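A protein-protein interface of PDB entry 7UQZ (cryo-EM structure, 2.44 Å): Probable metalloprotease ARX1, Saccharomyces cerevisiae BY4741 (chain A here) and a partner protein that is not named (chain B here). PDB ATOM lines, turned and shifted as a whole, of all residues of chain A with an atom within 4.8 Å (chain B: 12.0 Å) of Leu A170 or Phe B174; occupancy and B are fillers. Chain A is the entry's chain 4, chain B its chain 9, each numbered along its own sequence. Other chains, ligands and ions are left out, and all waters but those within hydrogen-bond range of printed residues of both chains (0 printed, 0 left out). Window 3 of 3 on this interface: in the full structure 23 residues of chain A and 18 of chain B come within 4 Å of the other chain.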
ATOM      1  N   ASN A  47      -8.480  36.381  28.072  1.00  0.00           N
ATOM      2  CA  ASN A  47      -9.126  35.082  28.238  1.00  0.00           C
ATOM      3  C   ASN A  47     -10.278  35.152  29.231  1.00  0.00           C
ATOM      4  O   ASN A  47     -11.328  34.534  29.018  1.00  0.00           O
ATOM      5  CB  ASN A  47      -8.102  34.037  28.681  1.00  0.00           C
ATOM      6  CG  ASN A  47      -7.174  33.623  27.559  1.00  0.00           C
ATOM      7  OD1 ASN A  47      -7.571  33.567  26.396  1.00  0.00           O
ATOM      8  ND2 ASN A  47      -5.927  33.328  27.903  1.00  0.00           N
ATOM      9  N   HIS A  51     -13.119  34.600  26.678  1.00  0.00           N
ATOM     10  CA  HIS A  51     -13.055  33.157  26.487  1.00  0.00           C
ATOM     11  C   HIS A  51     -13.622  32.387  27.673  1.00  0.00           C
ATOM     12  O   HIS A  51     -14.530  31.571  27.502  1.00  0.00           O
ATOM     13  CB  HIS A  51     -11.610  32.731  26.203  1.00  0.00           C
ATOM     14  CG  HIS A  51     -11.097  33.203  24.879  1.00  0.00           C
ATOM     15  ND1 HIS A  51      -9.757  33.405  24.628  1.00  0.00           N
ATOM     16  CD2 HIS A  51     -11.745  33.511  23.732  1.00  0.00           C
ATOM     17  CE1 HIS A  51      -9.602  33.820  23.384  1.00  0.00           C
ATOM     18  NE2 HIS A  51     -10.794  33.891  22.817  1.00  0.00           N
ATOM     19  N   SER A  52     -13.106  32.621  28.880  1.00  0.00           N
ATOM     20  CA  SER A  52     -13.663  31.950  30.048  1.00  0.00           C
ATOM     21  C   SER A  52     -15.034  32.504  30.410  1.00  0.00           C
ATOM     22  O   SER A  52     -15.880  31.767  30.932  1.00  0.00           O
ATOM     23  CB  SER A  52     -12.708  32.075  31.234  1.00  0.00           C
ATOM     24  OG  SER A  52     -11.469  31.444  30.960  1.00  0.00           O
ATOM     25  N   TYR A 161     -11.896  33.315  19.905  1.00  0.00           N
ATOM     26  CA  TYR A 161     -12.719  32.176  19.525  1.00  0.00           C
ATOM     27  C   TYR A 161     -14.094  32.241  20.181  1.00  0.00           C
ATOM     28  O   TYR A 161     -14.250  32.835  21.252  1.00  0.00           O
ATOM     29  CB  TYR A 161     -12.057  30.852  19.928  1.00  0.00           C
ATOM     30  CG  TYR A 161     -10.762  30.550  19.222  1.00  0.00           C
ATOM     31  CD1 TYR A 161     -10.758  29.972  17.959  1.00  0.00           C
ATOM     32  CD2 TYR A 161      -9.543  30.824  19.823  1.00  0.00           C
ATOM     33  CE1 TYR A 161      -9.576  29.689  17.313  1.00  0.00           C
ATOM     34  CE2 TYR A 161      -8.356  30.542  19.185  1.00  0.00           C
ATOM     35  CZ  TYR A 161      -8.379  29.974  17.930  1.00  0.00           C
ATOM     36  OH  TYR A 161      -7.196  29.695  17.289  1.00  0.00           O
ATOM     37  N   PRO A 162     -15.108  31.643  19.560  1.00  0.00           N
ATOM     38  CA  PRO A 162     -16.358  31.382  20.277  1.00  0.00           C
ATOM     39  C   PRO A 162     -16.181  30.249  21.277  1.00  0.00           C
ATOM     40  O   PRO A 162     -15.328  29.372  21.125  1.00  0.00           O
ATOM     41  CB  PRO A 162     -17.336  30.996  19.163  1.00  0.00           C
ATOM     42  CG  PRO A 162     -16.466  30.452  18.087  1.00  0.00           C
ATOM     43  CD  PRO A 162     -15.194  31.250  18.143  1.00  0.00           C
ATOM     44  N   VAL A 163     -17.014  30.274  22.313  1.00  0.00           N
ATOM     45  CA  VAL A 163     -16.883  29.374  23.454  1.00  0.00           C
ATOM     46  C   VAL A 163     -17.825  28.193  23.275  1.00  0.00           C
ATOM     47  O   VAL A 163     -19.016  28.374  22.991  1.00  0.00           O
ATOM     48  CB  VAL A 163     -17.172  30.109  24.773  1.00  0.00           C
ATOM     49  CG1 VAL A 163     -16.873  29.209  25.961  1.00  0.00           C
ATOM     50  CG2 VAL A 163     -16.364  31.392  24.845  1.00  0.00           C
ATOM     51  N   PRO A 168     -17.370  20.138  29.197  1.00  0.00           N
ATOM     52  CA  PRO A 168     -17.169  20.569  30.591  1.00  0.00           C
ATOM     53  C   PRO A 168     -16.047  21.578  30.756  1.00  0.00           C
ATOM     54  O   PRO A 168     -16.076  22.377  31.699  1.00  0.00           O
ATOM     55  CB  PRO A 168     -16.855  19.255  31.322  1.00  0.00           C
ATOM     56  CG  PRO A 168     -17.394  18.178  30.433  1.00  0.00           C
ATOM     57  CD  PRO A 168     -17.202  18.684  29.038  1.00  0.00           C
ATOM     58  N   ILE A 169     -15.057  21.563  29.868  1.00  0.00           N
ATOM     59  CA  ILE A 169     -13.878  22.413  29.964  1.00  0.00           C
ATOM     60  C   ILE A 169     -13.975  23.501  28.904  1.00  0.00           C
ATOM     61  O   ILE A 169     -14.383  23.236  27.766  1.00  0.00           O
ATOM     62  CB  ILE A 169     -12.586  21.587  29.802  1.00  0.00           C
ATOM     63  CG1 ILE A 169     -12.544  20.466  30.842  1.00  0.00           C
ATOM     64  CG2 ILE A 169     -11.350  22.469  29.918  1.00  0.00           C
ATOM     65  CD1 ILE A 169     -11.323  19.578  30.740  1.00  0.00           C
ATOM     66  N   LEU A 170     -13.622  24.729  29.287  1.00  0.00           N
ATOM     67  CA  LEU A 170     -13.622  25.859  28.364  1.00  0.00           C
ATOM     68  C   LEU A 170     -12.614  25.608  27.249  1.00  0.00           C
ATOM     69  O   LEU A 170     -11.402  25.578  27.490  1.00  0.00           O
ATOM     70  CB  LEU A 170     -13.295  27.154  29.104  1.00  0.00           C
ATOM     71  CG  LEU A 170     -14.364  27.811  29.986  1.00  0.00           C
ATOM     72  CD1 LEU A 170     -15.716  27.821  29.284  1.00  0.00           C
ATOM     73  CD2 LEU A 170     -14.459  27.157  31.361  1.00  0.00           C
ATOM     74  N   GLN A 171     -13.110  25.417  26.033  1.00  0.00           N
ATOM     75  CA  GLN A 171     -12.263  25.210  24.870  1.00  0.00           C
ATOM     76  C   GLN A 171     -12.955  25.818  23.661  1.00  0.00           C
ATOM     77  O   GLN A 171     -14.179  25.994  23.667  1.00  0.00           O
ATOM     78  CB  GLN A 171     -11.976  23.717  24.643  1.00  0.00           C
ATOM     79  CG  GLN A 171     -13.191  22.874  24.312  1.00  0.00           C
ATOM     80  CD  GLN A 171     -12.808  21.486  23.831  1.00  0.00           C
ATOM     81  OE1 GLN A 171     -12.433  21.302  22.675  1.00  0.00           O
ATOM     82  NE2 GLN A 171     -12.894  20.507  24.721  1.00  0.00           N
ATOM     83  N   PRO A 172     -12.202  26.178  22.623  1.00  0.00           N
ATOM     84  CA  PRO A 172     -12.833  26.694  21.402  1.00  0.00           C
ATOM     85  C   PRO A 172     -13.677  25.636  20.710  1.00  0.00           C
ATOM     86  O   PRO A 172     -13.430  24.433  20.825  1.00  0.00           O
ATOM     87  CB  PRO A 172     -11.640  27.103  20.529  1.00  0.00           C
ATOM     88  CG  PRO A 172     -10.517  27.299  21.483  1.00  0.00           C
ATOM     89  CD  PRO A 172     -10.734  26.300  22.572  1.00  0.00           C
ATOM     90  N   LEU B 169      -1.385  24.263  14.270  1.00  0.00           N
ATOM     91  CA  LEU B 169      -0.740  24.758  15.475  1.00  0.00           C
ATOM     92  C   LEU B 169      -1.770  24.895  16.586  1.00  0.00           C
ATOM     93  O   LEU B 169      -2.968  25.048  16.335  1.00  0.00           O
ATOM     94  CB  LEU B 169      -0.050  26.107  15.229  1.00  0.00           C
ATOM     95  CG  LEU B 169       1.020  26.155  14.135  1.00  0.00           C
ATOM     96  CD1 LEU B 169       1.686  27.521  14.106  1.00  0.00           C
ATOM     97  CD2 LEU B 169       2.052  25.055  14.326  1.00  0.00           C
ATOM     98  N   GLY B 170      -1.289  24.833  17.824  1.00  0.00           N
ATOM     99  CA  GLY B 170      -2.164  24.959  18.968  1.00  0.00           C
ATOM    100  C   GLY B 170      -2.992  23.705  19.209  1.00  0.00           C
ATOM    101  O   GLY B 170      -2.734  22.627  18.675  1.00  0.00           O
ATOM    102  N   GLY B 171      -4.016  23.877  20.041  1.00  0.00           N
ATOM    103  CA  GLY B 171      -4.895  22.791  20.401  1.00  0.00           C
ATOM    104  C   GLY B 171      -6.217  23.281  20.952  1.00  0.00           C
ATOM    105  O   GLY B 171      -6.456  24.486  21.079  1.00  0.00           O
ATOM    106  N   PRO B 172      -7.107  22.350  21.296  1.00  0.00           N
ATOM    107  CA  PRO B 172      -8.439  22.743  21.779  1.00  0.00           C
ATOM    108  C   PRO B 172      -8.428  23.266  23.207  1.00  0.00           C
ATOM    109  O   PRO B 172      -8.954  22.618  24.117  1.00  0.00           O
ATOM    110  CB  PRO B 172      -9.244  21.444  21.664  1.00  0.00           C
ATOM    111  CG  PRO B 172      -8.229  20.368  21.819  1.00  0.00           C
ATOM    112  CD  PRO B 172      -6.964  20.888  21.190  1.00  0.00           C
ATOM    113  N   PHE B 173      -7.837  24.443  23.409  1.00  0.00           N
ATOM    114  CA  PHE B 173      -7.780  25.077  24.719  1.00  0.00           C
ATOM    115  C   PHE B 173      -7.446  26.548  24.527  1.00  0.00           C
ATOM    116  O   PHE B 173      -7.073  26.984  23.435  1.00  0.00           O
ATOM    117  CB  PHE B 173      -6.754  24.396  25.636  1.00  0.00           C
ATOM    118  CG  PHE B 173      -5.353  24.400  25.092  1.00  0.00           C
ATOM    119  CD1 PHE B 173      -4.935  23.415  24.210  1.00  0.00           C
ATOM    120  CD2 PHE B 173      -4.451  25.383  25.469  1.00  0.00           C
ATOM    121  CE1 PHE B 173      -3.649  23.417  23.707  1.00  0.00           C
ATOM    122  CE2 PHE B 173      -3.163  25.388  24.968  1.00  0.00           C
ATOM    123  CZ  PHE B 173      -2.762  24.405  24.089  1.00  0.00           C
ATOM    124  N   PHE B 174      -7.582  27.311  25.608  1.00  0.00           N
ATOM    125  CA  PHE B 174      -7.220  28.723  25.596  1.00  0.00           C
ATOM    126  C   PHE B 174      -5.883  28.910  26.297  1.00  0.00           C
ATOM    127  O   PHE B 174      -5.794  28.684  27.516  1.00  0.00           O
ATOM    128  CB  PHE B 174      -8.300  29.569  26.271  1.00  0.00           C
ATOM    129  CG  PHE B 174      -9.641  29.484  25.603  1.00  0.00           C
ATOM    130  CD1 PHE B 174      -9.846  30.061  24.361  1.00  0.00           C
ATOM    131  CD2 PHE B 174     -10.698  28.835  26.219  1.00  0.00           C
ATOM    132  CE1 PHE B 174     -11.079  29.987  23.742  1.00  0.00           C
ATOM    133  CE2 PHE B 174     -11.935  28.759  25.604  1.00  0.00           C
ATOM    134  CZ  PHE B 174     -12.124  29.337  24.366  1.00  0.00           C
ATOM    135  N   PRO B 175      -4.818  29.304  25.584  1.00  0.00           N
ATOM    136  CA  PRO B 175      -3.494  29.530  26.176  1.00  0.00           C
ATOM    137  C   PRO B 175      -3.489  30.660  27.201  1.00  0.00           C
ATOM    138  O   PRO B 175      -3.254  30.391  28.379  1.00  0.00           O
ATOM    139  CB  PRO B 175      -2.626  29.893  24.967  1.00  0.00           C
ATOM    140  CG  PRO B 175      -3.342  29.316  23.793  1.00  0.00           C
ATOM    141  CD  PRO B 175      -4.795  29.453  24.118  1.00  0.00           C
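ND1 of His A51 sits at hydrogen-bond distance from OD1 of Asn A47.
N of Ser A52 sits at hydrogen-bond distance from O of Asn A47, at 2.6 Å.
A ring nitrogen (NE2) of His A51 is in hydrogen-bond range of the backbone NH (N) of Tyr A161 (3.2 Å).
ND2 of Asn A47 touches C of Pro B175, 3.7 Å away.
Phe B174 touches His A51 (CD1 to ND1, 3.4 Å).
Leu A170 touches Phe B174 (O to CD2, 3.6 Å).
Pro B172 touches Gln A171 (O to CB, 3.3 Å).
N of Gln A171 touches CE2 of Phe B174 (3.6 Å).
CD of Pro A172 touches C of Pro B172, at 3.9 Å.
Phe B173 touches Pro A172.
Phe B174 touches Pro A172 (CE1 to CG, 3.6 Å).
Printed residues of chain B within 4 Å of His A51: Phe B174.
No residue of chain B comes within 4 Å of Pro A162.
No residue of chain B comes within 4 Å of Val A163.
No residue of chain B comes within 4 Å of Ile A169.
Of chain B, only Phe B174 comes within 4 Å of Leu A170.
Gln A171 touches just these residues of chain B: Pro B172 (3.3 Å) and Phe B174 (3.6 Å).
Pro A172 touches three residues of chain B.
Leu B169 touches none of the printed residues of chain A.
Of the printed residues of chain A, Pro B172 touches Gln A171 and Pro A172.
Of the printed residues of chain A, Phe B173 touches Pro A172 (3.5 Å).
Phe B174 touches four residues of chain A.
The nearest printed residue of chain A that does not touch Phe B173 is Gln A171 (4.4 Å).
Hydrophobic or aromatic side chains of chain B that line the printed part of chain A: Pro B172 and Phe B174.
Among the printed residues, 8 pairs touch across the chains.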
